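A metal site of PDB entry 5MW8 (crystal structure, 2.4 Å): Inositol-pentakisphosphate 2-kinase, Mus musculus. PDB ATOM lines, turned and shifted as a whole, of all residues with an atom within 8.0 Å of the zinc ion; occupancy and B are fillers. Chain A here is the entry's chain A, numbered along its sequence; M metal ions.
The zinc ion is bound by SG of Cys 162 (2.0 Å), SG of Cys 184 (2.4 Å), SG of Cys 294 (2.4 Å) and SG of Cys 165 (2.5 Å).
Within 4 Å of the zinc ion: Cys 162, Cys 165, Cys 184 and Cys 294. The nearest printed residue that does not touch the zinc ion is Ser 297 (4.2 Å).
SG of Cys 184 sits close to N of Leu 186. N of Ala 296 sits close to SG of Cys 294, 3.4 Å away. SG of Cys 165 sits close to O of Tyr 183, at 3.6 Å.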
ATOM      1  N   CYS A 144      -2.454  20.960 -13.225  1.00  0.00           N
ATOM      2  CA  CYS A 144      -3.712  21.445 -13.795  1.00  0.00           C
ATOM      3  C   CYS A 144      -3.551  22.125 -15.144  1.00  0.00           C
ATOM      4  O   CYS A 144      -2.773  23.073 -15.274  1.00  0.00           O
ATOM      5  CB  CYS A 144      -4.395  22.424 -12.851  1.00  0.00           C
ATOM      6  SG  CYS A 144      -6.050  22.811 -13.419  1.00  0.00           S
ATOM      7  N   ILE A 147      -6.813  27.384 -16.780  1.00  0.00           N
ATOM      8  CA  ILE A 147      -6.874  28.553 -15.911  1.00  0.00           C
ATOM      9  C   ILE A 147      -8.330  28.740 -15.477  1.00  0.00           C
ATOM     10  O   ILE A 147      -9.229  28.694 -16.329  1.00  0.00           O
ATOM     11  CB  ILE A 147      -6.322  29.796 -16.651  1.00  0.00           C
ATOM     12  CG1 ILE A 147      -4.818  29.635 -16.877  1.00  0.00           C
ATOM     13  CG2 ILE A 147      -6.554  31.072 -15.854  1.00  0.00           C
ATOM     14  CD1 ILE A 147      -4.189  30.723 -17.722  1.00  0.00           C
ATOM     15  N   LYS A 160      -5.637  35.052 -15.173  1.00  0.00           N
ATOM     16  CA  LYS A 160      -4.540  35.385 -16.075  1.00  0.00           C
ATOM     17  C   LYS A 160      -3.401  34.362 -16.083  1.00  0.00           C
ATOM     18  O   LYS A 160      -2.923  33.973 -17.141  1.00  0.00           O
ATOM     19  CB  LYS A 160      -3.964  36.754 -15.705  1.00  0.00           C
ATOM     20  CG  LYS A 160      -4.963  37.894 -15.877  1.00  0.00           C
ATOM     21  CD  LYS A 160      -4.317  39.237 -15.550  1.00  0.00           C
ATOM     22  CE  LYS A 160      -4.975  40.399 -16.290  1.00  0.00           C
ATOM     23  NZ  LYS A 160      -4.038  41.541 -16.443  1.00  0.00           N
ATOM     24  N   VAL A 161      -2.974  33.946 -14.886  1.00  0.00           N
ATOM     25  CA  VAL A 161      -1.846  33.035 -14.712  1.00  0.00           C
ATOM     26  C   VAL A 161      -2.330  31.700 -14.137  1.00  0.00           C
ATOM     27  O   VAL A 161      -3.242  31.675 -13.305  1.00  0.00           O
ATOM     28  CB  VAL A 161      -0.778  33.656 -13.783  1.00  0.00           C
ATOM     29  CG1 VAL A 161       0.482  32.795 -13.742  1.00  0.00           C
ATOM     30  CG2 VAL A 161      -0.461  35.077 -14.230  1.00  0.00           C
ATOM     31  N   CYS A 162      -1.716  30.593 -14.565  1.00  0.00           N
ATOM     32  CA  CYS A 162      -2.079  29.267 -14.064  1.00  0.00           C
ATOM     33  C   CYS A 162      -1.627  29.086 -12.623  1.00  0.00           C
ATOM     34  O   CYS A 162      -0.738  29.783 -12.133  1.00  0.00           O
ATOM     35  CB  CYS A 162      -1.488  28.156 -14.933  1.00  0.00           C
ATOM     36  SG  CYS A 162       0.268  28.342 -15.311  1.00  0.00           S
ATOM     37  N   ARG A 163      -2.276  28.148 -11.950  1.00  0.00           N
ATOM     38  CA  ARG A 163      -1.930  27.763 -10.582  1.00  0.00           C
ATOM     39  C   ARG A 163      -0.448  27.415 -10.477  1.00  0.00           C
ATOM     40  O   ARG A 163       0.266  27.969  -9.647  1.00  0.00           O
ATOM     41  CB  ARG A 163      -2.816  26.571 -10.163  1.00  0.00           C
ATOM     42  CG  ARG A 163      -2.383  25.811  -8.922  1.00  0.00           C
ATOM     43  CD  ARG A 163      -2.268  26.688  -7.684  1.00  0.00           C
ATOM     44  NE  ARG A 163      -2.335  25.830  -6.505  1.00  0.00           N
ATOM     45  CZ  ARG A 163      -3.443  25.515  -5.823  1.00  0.00           C
ATOM     46  NH1 ARG A 163      -4.634  26.034  -6.135  1.00  0.00           N
ATOM     47  NH2 ARG A 163      -3.345  24.685  -4.787  1.00  0.00           N
ATOM     48  N   TYR A 164       0.004  26.502 -11.346  1.00  0.00           N
ATOM     49  CA  TYR A 164       1.387  26.025 -11.338  1.00  0.00           C
ATOM     50  C   TYR A 164       2.405  27.171 -11.385  1.00  0.00           C
ATOM     51  O   TYR A 164       3.238  27.285 -10.489  1.00  0.00           O
ATOM     52  CB  TYR A 164       1.637  25.053 -12.494  1.00  0.00           C
ATOM     53  CG  TYR A 164       3.025  24.461 -12.501  1.00  0.00           C
ATOM     54  CD1 TYR A 164       4.079  25.117 -13.126  1.00  0.00           C
ATOM     55  CD2 TYR A 164       3.284  23.254 -11.857  1.00  0.00           C
ATOM     56  CE1 TYR A 164       5.365  24.586 -13.113  1.00  0.00           C
ATOM     57  CE2 TYR A 164       4.562  22.711 -11.846  1.00  0.00           C
ATOM     58  CZ  TYR A 164       5.598  23.381 -12.480  1.00  0.00           C
ATOM     59  OH  TYR A 164       6.868  22.843 -12.466  1.00  0.00           O
ATOM     60  N   CYS A 165       2.336  28.006 -12.418  1.00  0.00           N
ATOM     61  CA  CYS A 165       3.307  29.085 -12.609  1.00  0.00           C
ATOM     62  C   CYS A 165       3.284  30.110 -11.476  1.00  0.00           C
ATOM     63  O   CYS A 165       4.330  30.622 -11.087  1.00  0.00           O
ATOM     64  CB  CYS A 165       3.113  29.786 -13.961  1.00  0.00           C
ATOM     65  SG  CYS A 165       3.493  28.731 -15.384  1.00  0.00           S
ATOM     66  N   MET A 166       2.088  30.394 -10.952  1.00  0.00           N
ATOM     67  CA  MET A 166       1.956  31.203  -9.734  1.00  0.00           C
ATOM     68  C   MET A 166       2.632  30.529  -8.534  1.00  0.00           C
ATOM     69  O   MET A 166       3.466  31.144  -7.863  1.00  0.00           O
ATOM     70  CB  MET A 166       0.492  31.473  -9.399  1.00  0.00           C
ATOM     71  CG  MET A 166      -0.146  32.586 -10.216  1.00  0.00           C
ATOM     72  SD  MET A 166      -1.588  33.290  -9.403  1.00  0.00           S
ATOM     73  CE  MET A 166      -2.692  31.880  -9.393  1.00  0.00           C
ATOM     74  N   SER A 181      10.604  27.228 -12.676  1.00  0.00           N
ATOM     75  CA  SER A 181      10.480  26.468 -13.913  1.00  0.00           C
ATOM     76  C   SER A 181       9.727  27.292 -14.950  1.00  0.00           C
ATOM     77  O   SER A 181       8.792  28.024 -14.604  1.00  0.00           O
ATOM     78  CB  SER A 181       9.742  25.147 -13.676  1.00  0.00           C
ATOM     79  OG  SER A 181       9.820  24.318 -14.817  1.00  0.00           O
ATOM     80  N   LYS A 182      10.140  27.163 -16.204  1.00  0.00           N
ATOM     81  CA  LYS A 182       9.468  27.810 -17.322  1.00  0.00           C
ATOM     82  C   LYS A 182       8.297  26.974 -17.833  1.00  0.00           C
ATOM     83  O   LYS A 182       7.503  27.446 -18.655  1.00  0.00           O
ATOM     84  CB  LYS A 182      10.452  28.054 -18.472  1.00  0.00           C
ATOM     85  CG  LYS A 182      11.659  28.885 -18.090  1.00  0.00           C
ATOM     86  CD  LYS A 182      12.520  29.193 -19.305  1.00  0.00           C
ATOM     87  CE  LYS A 182      13.962  29.467 -18.917  1.00  0.00           C
ATOM     88  NZ  LYS A 182      14.079  30.619 -17.983  1.00  0.00           N
ATOM     89  N   TYR A 183       8.198  25.728 -17.370  1.00  0.00           N
ATOM     90  CA  TYR A 183       7.056  24.870 -17.672  1.00  0.00           C
ATOM     91  C   TYR A 183       5.758  25.533 -17.229  1.00  0.00           C
ATOM     92  O   TYR A 183       5.629  25.950 -16.085  1.00  0.00           O
ATOM     93  CB  TYR A 183       7.200  23.505 -16.975  1.00  0.00           C
ATOM     94  CG  TYR A 183       5.977  22.618 -17.096  1.00  0.00           C
ATOM     95  CD1 TYR A 183       5.691  21.966 -18.290  1.00  0.00           C
ATOM     96  CD2 TYR A 183       5.105  22.443 -16.022  1.00  0.00           C
ATOM     97  CE1 TYR A 183       4.569  21.156 -18.404  1.00  0.00           C
ATOM     98  CE2 TYR A 183       3.988  21.637 -16.129  1.00  0.00           C
ATOM     99  CZ  TYR A 183       3.718  20.991 -17.323  1.00  0.00           C
ATOM    100  OH  TYR A 183       2.615  20.193 -17.445  1.00  0.00           O
ATOM    101  N   CYS A 184       4.840  25.663 -18.176  1.00  0.00           N
ATOM    102  CA  CYS A 184       3.462  26.035 -17.907  1.00  0.00           C
ATOM    103  C   CYS A 184       2.592  24.871 -18.408  1.00  0.00           C
ATOM    104  O   CYS A 184       2.758  24.454 -19.549  1.00  0.00           O
ATOM    105  CB  CYS A 184       3.104  27.302 -18.656  1.00  0.00           C
ATOM    106  SG  CYS A 184       1.343  27.714 -18.586  1.00  0.00           S
ATOM    107  N   PRO A 185       1.693  24.337 -17.557  1.00  0.00           N
ATOM    108  CA  PRO A 185       0.869  23.206 -18.014  1.00  0.00           C
ATOM    109  C   PRO A 185       0.024  23.493 -19.255  1.00  0.00           C
ATOM    110  O   PRO A 185      -0.168  22.588 -20.073  1.00  0.00           O
ATOM    111  CB  PRO A 185      -0.036  22.913 -16.819  1.00  0.00           C
ATOM    112  CG  PRO A 185       0.714  23.438 -15.644  1.00  0.00           C
ATOM    113  CD  PRO A 185       1.467  24.641 -16.130  1.00  0.00           C
ATOM    114  N   LEU A 186      -0.457  24.723 -19.412  1.00  0.00           N
ATOM    115  CA  LEU A 186      -1.254  25.091 -20.586  1.00  0.00           C
ATOM    116  C   LEU A 186      -0.503  24.986 -21.921  1.00  0.00           C
ATOM    117  O   LEU A 186      -1.141  24.838 -22.969  1.00  0.00           O
ATOM    118  CB  LEU A 186      -1.841  26.505 -20.446  1.00  0.00           C
ATOM    119  CG  LEU A 186      -3.149  26.575 -19.634  1.00  0.00           C
ATOM    120  CD1 LEU A 186      -2.897  26.424 -18.143  1.00  0.00           C
ATOM    121  CD2 LEU A 186      -3.873  27.880 -19.916  1.00  0.00           C
ATOM    122  N   ASP A 187       0.834  25.046 -21.899  1.00  0.00           N
ATOM    123  CA  ASP A 187       1.637  24.755 -23.088  1.00  0.00           C
ATOM    124  C   ASP A 187       1.577  23.272 -23.452  1.00  0.00           C
ATOM    125  O   ASP A 187       1.420  22.916 -24.616  1.00  0.00           O
ATOM    126  CB  ASP A 187       3.110  25.171 -22.888  1.00  0.00           C
ATOM    127  CG  ASP A 187       3.305  26.684 -22.740  1.00  0.00           C
ATOM    128  OD1 ASP A 187       2.438  27.481 -23.170  1.00  0.00           O
ATOM    129  OD2 ASP A 187       4.351  27.079 -22.200  1.00  0.00           O
ATOM    130  N   ARG A 195       4.420  24.561 -28.671  1.00  0.00           N
ATOM    131  CA  ARG A 195       4.191  24.824 -27.244  1.00  0.00           C
ATOM    132  C   ARG A 195       4.518  23.588 -26.412  1.00  0.00           C
ATOM    133  O   ARG A 195       5.181  23.703 -25.374  1.00  0.00           O
ATOM    134  CB  ARG A 195       2.744  25.244 -26.985  1.00  0.00           C
ATOM    135  CG  ARG A 195       2.355  26.588 -27.585  1.00  0.00           C
ATOM    136  CD  ARG A 195       0.937  26.987 -27.210  1.00  0.00           C
ATOM    137  NE  ARG A 195       0.772  27.170 -25.764  1.00  0.00           N
ATOM    138  CZ  ARG A 195      -0.369  27.521 -25.155  1.00  0.00           C
ATOM    139  NH1 ARG A 195      -1.476  27.751 -25.861  1.00  0.00           N
ATOM    140  NH2 ARG A 195      -0.394  27.654 -23.840  1.00  0.00           N
ATOM    141  N   VAL A 293      -3.859  30.442 -23.208  1.00  0.00           N
ATOM    142  CA  VAL A 293      -2.479  30.854 -23.024  1.00  0.00           C
ATOM    143  C   VAL A 293      -2.349  31.538 -21.665  1.00  0.00           C
ATOM    144  O   VAL A 293      -3.185  32.373 -21.300  1.00  0.00           O
ATOM    145  CB  VAL A 293      -2.007  31.793 -24.173  1.00  0.00           C
ATOM    146  CG1 VAL A 293      -0.635  32.390 -23.882  1.00  0.00           C
ATOM    147  CG2 VAL A 293      -1.976  31.037 -25.490  1.00  0.00           C
ATOM    148  N   CYS A 294      -1.299  31.174 -20.933  1.00  0.00           N
ATOM    149  CA  CYS A 294      -0.997  31.744 -19.619  1.00  0.00           C
ATOM    150  C   CYS A 294       0.006  32.875 -19.770  1.00  0.00           C
ATOM    151  O   CYS A 294       0.935  32.781 -20.568  1.00  0.00           O
ATOM    152  CB  CYS A 294      -0.406  30.656 -18.717  1.00  0.00           C
ATOM    153  SG  CYS A 294       0.260  31.229 -17.151  1.00  0.00           S
ATOM    154  N   GLU A 295      -0.171  33.942 -18.991  1.00  0.00           N
ATOM    155  CA  GLU A 295       0.731  35.098 -19.035  1.00  0.00           C
ATOM    156  C   GLU A 295       2.137  34.783 -18.519  1.00  0.00           C
ATOM    157  O   GLU A 295       3.116  35.318 -19.033  1.00  0.00           O
ATOM    158  CB  GLU A 295       0.166  36.286 -18.257  1.00  0.00           C
ATOM    159  CG  GLU A 295      -1.047  36.928 -18.913  1.00  0.00           C
ATOM    160  CD  GLU A 295      -1.501  38.211 -18.229  1.00  0.00           C
ATOM    161  OE1 GLU A 295      -0.731  38.791 -17.439  1.00  0.00           O
ATOM    162  OE2 GLU A 295      -2.649  38.644 -18.490  1.00  0.00           O
ATOM    163  N   ALA A 296       2.228  33.918 -17.511  1.00  0.00           N
ATOM    164  CA  ALA A 296       3.527  33.518 -16.953  1.00  0.00           C
ATOM    165  C   ALA A 296       4.349  32.632 -17.885  1.00  0.00           C
ATOM    166  O   ALA A 296       5.570  32.580 -17.744  1.00  0.00           O
ATOM    167  CB  ALA A 296       3.337  32.815 -15.611  1.00  0.00           C
ATOM    168  N   SER A 297       3.694  31.952 -18.826  1.00  0.00           N
ATOM    169  CA  SER A 297       4.383  31.112 -19.818  1.00  0.00           C
ATOM    170  C   SER A 297       5.274  31.957 -20.733  1.00  0.00           C
ATOM    171  O   SER A 297       4.759  32.821 -21.440  1.00  0.00           O
ATOM    172  CB  SER A 297       3.370  30.351 -20.658  1.00  0.00           C
ATOM    173  OG  SER A 297       4.021  29.532 -21.611  1.00  0.00           O
ATOM    174  N   PRO A 298       6.612  31.725 -20.722  1.00  0.00           N
ATOM    175  CA  PRO A 298       7.519  32.528 -21.567  1.00  0.00           C
ATOM    176  C   PRO A 298       7.294  32.395 -23.079  1.00  0.00           C
ATOM    177  O   PRO A 298       7.528  31.330 -23.654  1.00  0.00           O
ATOM    178  CB  PRO A 298       8.927  32.024 -21.168  1.00  0.00           C
ATOM    179  CG  PRO A 298       8.745  31.411 -19.832  1.00  0.00           C
ATOM    180  CD  PRO A 298       7.375  30.813 -19.841  1.00  0.00           C
ATOM    181  N   TYR A 463       2.240  35.779  -5.055  1.00  0.00           N
ATOM    182  CA  TYR A 463       2.514  36.060  -6.466  1.00  0.00           C
ATOM    183  C   TYR A 463       2.213  37.517  -6.788  1.00  0.00           C
ATOM    184  O   TYR A 463       3.028  38.198  -7.403  1.00  0.00           O
ATOM    185  CB  TYR A 463       1.706  35.140  -7.387  1.00  0.00           C
ATOM    186  CG  TYR A 463       1.994  35.340  -8.867  1.00  0.00           C
ATOM    187  CD1 TYR A 463       3.104  34.751  -9.458  1.00  0.00           C
ATOM    188  CD2 TYR A 463       1.159  36.131  -9.666  1.00  0.00           C
ATOM    189  CE1 TYR A 463       3.390  34.932 -10.802  1.00  0.00           C
ATOM    190  CE2 TYR A 463       1.432  36.312 -11.015  1.00  0.00           C
ATOM    191  CZ  TYR A 463       2.542  35.713 -11.586  1.00  0.00           C
ATOM    192  OH  TYR A 463       2.817  35.892 -12.922  1.00  0.00           O
HETATM  193 ZN    ZN M   1       1.406  29.148 -16.720  1.00  0.00          ZN
